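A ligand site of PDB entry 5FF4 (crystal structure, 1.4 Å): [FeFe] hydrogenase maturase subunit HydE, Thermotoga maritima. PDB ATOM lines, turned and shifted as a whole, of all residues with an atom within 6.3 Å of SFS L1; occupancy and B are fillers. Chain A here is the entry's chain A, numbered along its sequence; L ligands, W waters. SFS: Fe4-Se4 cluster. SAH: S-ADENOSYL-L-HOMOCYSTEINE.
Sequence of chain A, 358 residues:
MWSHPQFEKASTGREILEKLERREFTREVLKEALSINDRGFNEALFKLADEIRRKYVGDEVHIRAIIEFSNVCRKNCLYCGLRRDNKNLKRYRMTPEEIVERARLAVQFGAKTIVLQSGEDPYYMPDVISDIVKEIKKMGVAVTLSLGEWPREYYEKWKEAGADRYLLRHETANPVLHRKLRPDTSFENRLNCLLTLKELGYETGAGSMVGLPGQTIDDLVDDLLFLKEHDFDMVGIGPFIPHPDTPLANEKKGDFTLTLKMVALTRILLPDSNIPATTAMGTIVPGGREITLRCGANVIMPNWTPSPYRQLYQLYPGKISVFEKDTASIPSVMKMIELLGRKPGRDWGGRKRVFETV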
ATOM      1  N   VAL A  72      26.680   4.938   2.763  1.00  0.00           N
ATOM      2  CA  VAL A  72      25.477   4.689   3.607  1.00  0.00           C
ATOM      3  C   VAL A  72      24.391   4.143   2.691  1.00  0.00           C
ATOM      4  O   VAL A  72      24.132   4.655   1.610  1.00  0.00           O
ATOM      5  CB  VAL A  72      25.010   5.970   4.280  1.00  0.00           C
ATOM      6  CG1 VAL A  72      23.640   5.785   4.971  1.00  0.00           C
ATOM      7  CG2 VAL A  72      26.086   6.493   5.255  1.00  0.00           C
ATOM      8  N   CYS A  73      23.728   3.038   3.125  1.00  0.00           N
ATOM      9  CA  CYS A  73      22.608   2.520   2.390  1.00  0.00           C
ATOM     10  C   CYS A  73      21.448   2.048   3.239  1.00  0.00           C
ATOM     11  O   CYS A  73      21.679   1.393   4.245  1.00  0.00           O
ATOM     12  CB  CYS A  73      23.006   1.333   1.450  1.00  0.00           C
ATOM     13  SG  CYS A  73      21.754   1.047   0.166  1.00  0.00           S
ATOM     14  N   ARG A  74      20.249   2.375   2.839  1.00  0.00           N
ATOM     15  CA  ARG A  74      19.002   1.972   3.539  1.00  0.00           C
ATOM     16  C   ARG A  74      18.523   0.563   3.099  1.00  0.00           C
ATOM     17  O   ARG A  74      17.643  -0.019   3.764  1.00  0.00           O
ATOM     18  CB  ARG A  74      17.897   2.935   3.239  1.00  0.00           C
ATOM     19  CG  ARG A  74      17.404   2.985   1.840  1.00  0.00           C
ATOM     20  CD  ARG A  74      16.433   4.006   1.578  1.00  0.00           C
ATOM     21  NE  ARG A  74      16.045   4.142   0.189  1.00  0.00           N
ATOM     22  CZ  ARG A  74      14.991   4.739  -0.276  1.00  0.00           C
ATOM     23  NH1 ARG A  74      14.186   5.400   0.516  1.00  0.00           N
ATOM     24  NH2 ARG A  74      14.746   4.750  -1.588  1.00  0.00           N
ATOM     25  N   LYS A  75      19.014   0.013   1.973  1.00  0.00           N
ATOM     26  CA  LYS A  75      18.585  -1.277   1.454  1.00  0.00           C
ATOM     27  C   LYS A  75      19.542  -2.367   1.948  1.00  0.00           C
ATOM     28  O   LYS A  75      20.551  -2.139   2.526  1.00  0.00           O
ATOM     29  CB  LYS A  75      18.490  -1.227  -0.060  1.00  0.00           C
ATOM     30  CG  LYS A  75      17.196  -0.596  -0.567  1.00  0.00           C
ATOM     31  CD  LYS A  75      17.028  -0.704  -2.044  1.00  0.00           C
ATOM     32  CE  LYS A  75      15.670  -0.341  -2.576  1.00  0.00           C
ATOM     33  NZ  LYS A  75      15.131   0.968  -2.103  1.00  0.00           N
ATOM     34  N   ASN A  76      19.106  -3.632   1.671  1.00  0.00           N
ATOM     35  CA  ASN A  76      19.737  -4.799   2.253  1.00  0.00           C
ATOM     36  C   ASN A  76      19.966  -5.888   1.216  1.00  0.00           C
ATOM     37  O   ASN A  76      19.876  -7.076   1.500  1.00  0.00           O
ATOM     38  CB  ASN A  76      18.876  -5.350   3.402  1.00  0.00           C
ATOM     39  CG  ASN A  76      19.701  -5.972   4.487  1.00  0.00           C
ATOM     40  OD1 ASN A  76      20.839  -5.701   4.752  1.00  0.00           O
ATOM     41  ND2 ASN A  76      18.991  -6.852   5.275  1.00  0.00           N
ATOM     42  N   CYS A  77      20.241  -5.500  -0.010  1.00  0.00           N
ATOM     43  CA  CYS A  77      20.501  -6.496  -1.072  1.00  0.00           C
ATOM     44  C   CYS A  77      21.501  -7.511  -0.610  1.00  0.00           C
ATOM     45  O   CYS A  77      22.508  -7.272  -0.010  1.00  0.00           O
ATOM     46  CB  CYS A  77      21.067  -5.764  -2.320  1.00  0.00           C
ATOM     47  SG  CYS A  77      20.048  -4.329  -2.877  1.00  0.00           S
ATOM     48  N   TYR A  79      23.578  -9.476  -2.038  1.00  0.00           N
ATOM     49  CA  TYR A  79      24.912  -9.580  -2.609  1.00  0.00           C
ATOM     50  C   TYR A  79      25.857  -8.494  -2.268  1.00  0.00           C
ATOM     51  O   TYR A  79      27.070  -8.634  -2.491  1.00  0.00           O
ATOM     52  CB  TYR A  79      24.758  -9.604  -4.116  1.00  0.00           C
ATOM     53  CG  TYR A  79      23.827  -8.630  -4.707  1.00  0.00           C
ATOM     54  CD1 TYR A  79      24.210  -7.268  -4.903  1.00  0.00           C
ATOM     55  CD2 TYR A  79      22.544  -8.936  -5.075  1.00  0.00           C
ATOM     56  CE1 TYR A  79      23.342  -6.371  -5.428  1.00  0.00           C
ATOM     57  CE2 TYR A  79      21.639  -8.042  -5.560  1.00  0.00           C
ATOM     58  CZ  TYR A  79      22.072  -6.697  -5.709  1.00  0.00           C
ATOM     59  OH  TYR A  79      21.179  -5.821  -6.202  1.00  0.00           O
ATOM     60  N   CYS A  80      25.409  -7.422  -1.672  1.00  0.00           N
ATOM     61  CA  CYS A  80      26.194  -6.157  -1.631  1.00  0.00           C
ATOM     62  C   CYS A  80      26.886  -5.902  -0.330  1.00  0.00           C
ATOM     63  O   CYS A  80      26.187  -5.908   0.731  1.00  0.00           O
ATOM     64  CB  CYS A  80      25.284  -4.995  -1.903  1.00  0.00           C
ATOM     65  SG  CYS A  80      26.120  -3.416  -2.059  1.00  0.00           S
ATOM     66  N   GLY A  81      28.159  -5.559  -0.310  1.00  0.00           N
ATOM     67  CA  GLY A  81      28.827  -5.201   0.877  1.00  0.00           C
ATOM     68  C   GLY A  81      28.382  -3.962   1.616  1.00  0.00           C
ATOM     69  O   GLY A  81      28.684  -3.786   2.795  1.00  0.00           O
ATOM     70  N   LEU A  82      27.623  -3.087   0.955  1.00  0.00           N
ATOM     71  CA  LEU A  82      27.072  -1.907   1.581  1.00  0.00           C
ATOM     72  C   LEU A  82      25.668  -2.104   2.186  1.00  0.00           C
ATOM     73  O   LEU A  82      25.158  -1.199   2.768  1.00  0.00           O
ATOM     74  CB  LEU A  82      27.008  -0.699   0.595  1.00  0.00           C
ATOM     75  CG  LEU A  82      28.348  -0.275   0.000  1.00  0.00           C
ATOM     76  CD1 LEU A  82      28.095   1.066  -0.792  1.00  0.00           C
ATOM     77  CD2 LEU A  82      29.549  -0.370   0.674  1.00  0.00           C
ATOM     78  N   ARG A  83      25.164  -3.321   2.124  1.00  0.00           N
ATOM     79  CA  ARG A  83      23.862  -3.616   2.689  1.00  0.00           C
ATOM     80  C   ARG A  83      23.788  -3.128   4.123  1.00  0.00           C
ATOM     81  O   ARG A  83      24.721  -3.215   4.901  1.00  0.00           O
ATOM     82  CB  ARG A  83      23.515  -5.116   2.568  1.00  0.00           C
ATOM     83  CG  ARG A  83      24.405  -6.026   3.404  1.00  0.00           C
ATOM     84  CD  ARG A  83      24.306  -7.461   2.936  1.00  0.00           C
ATOM     85  NE  ARG A  83      22.956  -7.907   2.787  1.00  0.00           N
ATOM     86  CZ  ARG A  83      22.215  -8.511   3.748  1.00  0.00           C
ATOM     87  NH1 ARG A  83      22.772  -8.768   4.917  1.00  0.00           N
ATOM     88  NH2 ARG A  83      20.979  -8.817   3.511  1.00  0.00           N
ATOM     89  N   ARG A  84      22.566  -2.703   4.485  1.00  0.00           N
ATOM     90  CA  ARG A  84      22.425  -2.087   5.825  1.00  0.00           C
ATOM     91  C   ARG A  84      22.772  -2.974   7.005  1.00  0.00           C
ATOM     92  O   ARG A  84      23.219  -2.448   8.009  1.00  0.00           O
ATOM     93  CB  ARG A  84      21.039  -1.497   6.043  1.00  0.00           C
ATOM     94  CG  ARG A  84      19.911  -2.445   6.099  1.00  0.00           C
ATOM     95  CD  ARG A  84      18.594  -1.758   6.570  1.00  0.00           C
ATOM     96  NE  ARG A  84      17.666  -2.861   6.655  1.00  0.00           N
ATOM     97  CZ  ARG A  84      16.829  -3.253   5.717  1.00  0.00           C
ATOM     98  NH1 ARG A  84      16.691  -2.631   4.537  1.00  0.00           N
ATOM     99  NH2 ARG A  84      16.132  -4.394   5.873  1.00  0.00           N
ATOM    100  N   SER A 118      26.395   6.335  -5.080  1.00  0.00           N
ATOM    101  CA  SER A 118      26.321   6.150  -3.655  1.00  0.00           C
ATOM    102  C   SER A 118      25.448   4.966  -3.348  1.00  0.00           C
ATOM    103  O   SER A 118      24.674   4.470  -4.149  1.00  0.00           O
ATOM    104  CB  SER A 118      25.787   7.389  -2.934  1.00  0.00           C
ATOM    105  OG  SER A 118      24.475   7.701  -3.392  1.00  0.00           O
ATOM    106  N   GLY A 119      25.542   4.554  -2.058  1.00  0.00           N
ATOM    107  CA  GLY A 119      24.447   3.772  -1.459  1.00  0.00           C
ATOM    108  C   GLY A 119      23.160   4.606  -1.503  1.00  0.00           C
ATOM    109  O   GLY A 119      23.192   5.835  -1.750  1.00  0.00           O
ATOM    110  N   GLU A 120      22.039   4.008  -1.286  1.00  0.00           N
ATOM    111  CA  GLU A 120      20.794   4.755  -1.124  1.00  0.00           C
ATOM    112  C   GLU A 120      20.802   5.433   0.206  1.00  0.00           C
ATOM    113  O   GLU A 120      20.217   4.921   1.226  1.00  0.00           O
ATOM    114  CB  GLU A 120      19.559   3.862  -1.277  1.00  0.00           C
ATOM    115  CG  GLU A 120      19.376   3.349  -2.690  1.00  0.00           C
ATOM    116  CD  GLU A 120      18.002   2.737  -2.957  1.00  0.00           C
ATOM    117  OE1 GLU A 120      17.145   2.822  -2.044  1.00  0.00           O
ATOM    118  OE2 GLU A 120      17.802   2.171  -4.054  1.00  0.00           O
ATOM    119  N   GLY A 148      20.430   4.812  -7.058  1.00  0.00           N
ATOM    120  CA  GLY A 148      19.393   3.841  -6.700  1.00  0.00           C
ATOM    121  C   GLY A 148      17.979   4.324  -7.028  1.00  0.00           C
ATOM    122  O   GLY A 148      17.741   5.152  -7.905  1.00  0.00           O
ATOM    123  N   GLU A 171      19.814  -5.606 -12.698  1.00  0.00           N
ATOM    124  CA  GLU A 171      20.374  -6.620 -11.818  1.00  0.00           C
ATOM    125  C   GLU A 171      20.091  -8.080 -12.296  1.00  0.00           C
ATOM    126  O   GLU A 171      21.063  -8.810 -12.513  1.00  0.00           O
ATOM    127  CB  GLU A 171      19.976  -6.458 -10.329  1.00  0.00           C
ATOM    128  CG  GLU A 171      20.200  -5.034  -9.800  1.00  0.00           C
ATOM    129  CD  GLU A 171      21.596  -4.531  -9.789  1.00  0.00           C
ATOM    130  OE1 GLU A 171      22.490  -5.171 -10.276  1.00  0.00           O
ATOM    131  OE2 GLU A 171      21.723  -3.389  -9.243  1.00  0.00           O
ATOM    132  N   ARG A 182      16.831  -8.877  -3.485  1.00  0.00           N
ATOM    133  CA  ARG A 182      16.629  -7.435  -3.176  1.00  0.00           C
ATOM    134  C   ARG A 182      15.306  -7.302  -2.420  1.00  0.00           C
ATOM    135  O   ARG A 182      14.290  -6.904  -2.964  1.00  0.00           O
ATOM    136  CB  ARG A 182      16.620  -6.669  -4.491  1.00  0.00           C
ATOM    137  CG  ARG A 182      17.860  -6.962  -5.341  1.00  0.00           C
ATOM    138  CD  ARG A 182      18.031  -6.054  -6.542  1.00  0.00           C
ATOM    139  NE  ARG A 182      18.327  -4.668  -6.089  1.00  0.00           N
ATOM    140  CZ  ARG A 182      17.508  -3.673  -6.210  1.00  0.00           C
ATOM    141  NH1 ARG A 182      16.455  -3.665  -6.939  1.00  0.00           N
ATOM    142  NH2 ARG A 182      17.887  -2.553  -5.511  1.00  0.00           N
ATOM    143  N   ARG A 190      11.971  -1.681 -10.103  1.00  0.00           N
ATOM    144  CA  ARG A 190      13.195  -1.358 -10.818  1.00  0.00           C
ATOM    145  C   ARG A 190      12.925  -0.905 -12.203  1.00  0.00           C
ATOM    146  O   ARG A 190      13.445   0.113 -12.702  1.00  0.00           O
ATOM    147  CB  ARG A 190      14.122  -2.570 -10.745  1.00  0.00           C
ATOM    148  CG  ARG A 190      15.600  -2.328 -11.069  1.00  0.00           C
ATOM    149  CD  ARG A 190      16.236  -1.594  -9.879  1.00  0.00           C
ATOM    150  NE  ARG A 190      17.708  -1.587  -9.984  1.00  0.00           N
ATOM    151  CZ  ARG A 190      18.473  -0.944  -9.109  1.00  0.00           C
ATOM    152  NH1 ARG A 190      17.992  -0.448  -8.028  1.00  0.00           N
ATOM    153  NH2 ARG A 190      19.782  -0.915  -9.349  1.00  0.00           N
ATOM    154  N   TYR A 313      34.470   1.895   0.189  1.00  0.00           N
ATOM    155  CA  TYR A 313      33.364   1.662  -0.727  1.00  0.00           C
ATOM    156  C   TYR A 313      33.482   0.280  -1.342  1.00  0.00           C
ATOM    157  O   TYR A 313      33.918   0.095  -2.452  1.00  0.00           O
ATOM    158  CB  TYR A 313      33.240   2.689  -1.812  1.00  0.00           C
ATOM    159  CG  TYR A 313      31.890   2.743  -2.506  1.00  0.00           C
ATOM    160  CD1 TYR A 313      30.839   3.450  -2.043  1.00  0.00           C
ATOM    161  CD2 TYR A 313      31.695   2.051  -3.666  1.00  0.00           C
ATOM    162  CE1 TYR A 313      29.650   3.562  -2.711  1.00  0.00           C
ATOM    163  CE2 TYR A 313      30.514   2.156  -4.343  1.00  0.00           C
ATOM    164  CZ  TYR A 313      29.533   2.856  -3.836  1.00  0.00           C
ATOM    165  OH  TYR A 313      28.364   2.943  -4.522  1.00  0.00           O
ATOM    166  N   LEU A 315      31.550  -2.681  -2.466  1.00  0.00           N
ATOM    167  CA  LEU A 315      30.441  -3.437  -2.829  1.00  0.00           C
ATOM    168  C   LEU A 315      30.825  -4.930  -2.915  1.00  0.00           C
ATOM    169  O   LEU A 315      30.008  -5.734  -2.524  1.00  0.00           O
ATOM    170  CB  LEU A 315      29.975  -2.960  -4.233  1.00  0.00           C
ATOM    171  CG  LEU A 315      29.656  -1.515  -4.352  1.00  0.00           C
ATOM    172  CD1 LEU A 315      29.534  -1.233  -5.864  1.00  0.00           C
ATOM    173  CD2 LEU A 315      28.376  -1.199  -3.682  1.00  0.00           C
HETATM  174 SE4  SFS L   1      22.672  -2.638  -0.674  1.00  0.00          SE
HETATM  175 FE1  SFS L   1      24.268  -2.122  -2.412  1.00  0.00          FE
HETATM  176 FE3  SFS L   1      21.604  -2.625  -2.842  1.00  0.00          FE
HETATM  177 FE2  SFS L   1      22.514  -0.405  -1.377  1.00  0.00          FE
HETATM  178 SE3  SFS L   1      24.559   0.159  -2.406  1.00  0.00          SE
HETATM  179 FE4  SFS L   1      22.955  -0.341  -4.266  1.00  0.00          FE
HETATM  180 SE2  SFS L   1      23.326  -2.768  -4.504  1.00  0.00          SE
HETATM  181 SE1  SFS L   1      20.759  -0.385  -3.048  1.00  0.00          SE
HETATM  182  N   SAH L   2      22.956   1.815  -4.807  1.00  0.00           N
HETATM  183  CA  SAH L   2      22.944   2.110  -6.282  1.00  0.00           C
HETATM  184  CB  SAH L   2      24.391   2.306  -6.715  1.00  0.00           C
HETATM  185  CG  SAH L   2      25.544   1.525  -6.066  1.00  0.00           C
HETATM  186  SD  SAH L   2      25.509  -0.242  -6.302  1.00  0.00           S
HETATM  187  C   SAH L   2      22.300   0.941  -6.902  1.00  0.00           C
HETATM  188  O   SAH L   2      21.921   1.094  -8.118  1.00  0.00           O
HETATM  189  OXT SAH L   2      22.047  -0.159  -6.272  1.00  0.00           O
HETATM  190  C5' SAH L   2      25.952  -0.333  -8.044  1.00  0.00           C
HETATM  191  C4' SAH L   2      25.978  -1.769  -8.620  1.00  0.00           C
HETATM  192  O4' SAH L   2      26.938  -2.608  -7.912  1.00  0.00           O
HETATM  193  C3' SAH L   2      24.728  -2.607  -8.520  1.00  0.00           C
HETATM  194  O3' SAH L   2      23.810  -2.204  -9.528  1.00  0.00           O
HETATM  195  C2' SAH L   2      25.211  -4.087  -8.635  1.00  0.00           C
HETATM  196  O2' SAH L   2      25.035  -4.655  -9.925  1.00  0.00           O
HETATM  197  C1' SAH L   2      26.734  -3.979  -8.314  1.00  0.00           C
HETATM  198  N9  SAH L   2      27.170  -4.784  -7.234  1.00  0.00           N
HETATM  199  C8  SAH L   2      26.738  -4.698  -5.963  1.00  0.00           C
HETATM  200  N7  SAH L   2      27.261  -5.730  -5.213  1.00  0.00           N
HETATM  201  C5  SAH L   2      28.011  -6.525  -6.088  1.00  0.00           C
HETATM  202  C6  SAH L   2      28.786  -7.672  -5.921  1.00  0.00           C
HETATM  203  N6  SAH L   2      28.848  -8.333  -4.769  1.00  0.00           N
HETATM  204  N1  SAH L   2      29.393  -8.186  -7.027  1.00  0.00           N
HETATM  205  C2  SAH L   2      29.414  -7.507  -8.203  1.00  0.00           C
HETATM  206  N3  SAH L   2      28.665  -6.383  -8.406  1.00  0.00           N
HETATM  207  C4  SAH L   2      28.008  -5.855  -7.378  1.00  0.00           C
HETATM  208  O   HOH W   1      20.905  -3.046  -6.650  1.00  0.00           O
HETATM  209  O   HOH W   2      19.174   0.599  -5.737  1.00  0.00           O
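The side-chain sulfur (SG) of Cys 73 binds an iron atom (FE2) of SFS L1, 2.3 Å away. An oxygen (O3') of SAH L2 is in hydrogen-bond range of the side-chain carboxylate of Glu 171 (2.4 Å). The guanidinium group of Arg 190 lies within salt-bridge range of an oxygen (O) of SAH L2 (3.2 Å). N of SAH L2 lies close to O of Ser 118 (3.2 Å). An iron atom (FE1) of SFS L1 is bound by the side-chain sulfur (SG) of Cys 80 (2.3 Å). SG of Cys 77 is bound to FE3 of SFS L1. The backbone carbonyl oxygen (O) of Tyr 79 is in hydrogen-bond range of a nitrogen (N6) of SAH L2.
OXT of SAH L2 binds FE4 of SFS L1.
The guanidinium group (NH2) of Arg 83 sits at hydrogen-bond distance from the backbone carbonyl oxygen (O) of Asn 76 (2.9 Å). The guanidinium group (NE) of Arg 182 sits at hydrogen-bond distance from the side-chain hydroxyl (OH) of Tyr 79, 3.1 Å away. The side-chain carboxylate (OE1) of Glu 120 lies within salt-bridge range of the side-chain amino group (NZ) of Lys 75, 2.7 Å away. NE of Arg 83 sits at hydrogen-bond distance from O of Cys 77. N of Leu 82 sits close to SG of Cys 80. The side-chain carboxylate (OE1) of Glu 120 is in salt-bridge range of the guanidinium group (NE) of Arg 74. The backbone NH (N) of Lys 75 sits close to the side-chain sulfur (SG) of Cys 73 (3.4 Å). SG of Cys 77 sits close to NE of Arg 182 (3.7 Å).
Residues that only touch SFS L1: Arg 83 (3.7 Å), Tyr 79 (3.7 Å), Gly 119 (3.7 Å), Lys 75 (3.8 Å), Leu 82 (3.97 Å) and Glu 120 (3.998 Å). Hydrophobic or aromatic side chains within 4 Å of SFS L1: Tyr 79 and Leu 82. Of the 21 residues printed, 9 come within 4 Å of SFS L1.
Water W1 lies within hydrogen-bond range of OE2 of Glu 171 (2.7 Å), OH of Tyr 79 (2.8 Å) and NE of Arg 182 (3.1 Å). Water W2 lies within hydrogen-bond range of OE2 of Glu 120 (2.7 Å), NH1 of Arg 190 (2.8 Å) and NH2 of Arg 182 (3.4 Å).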
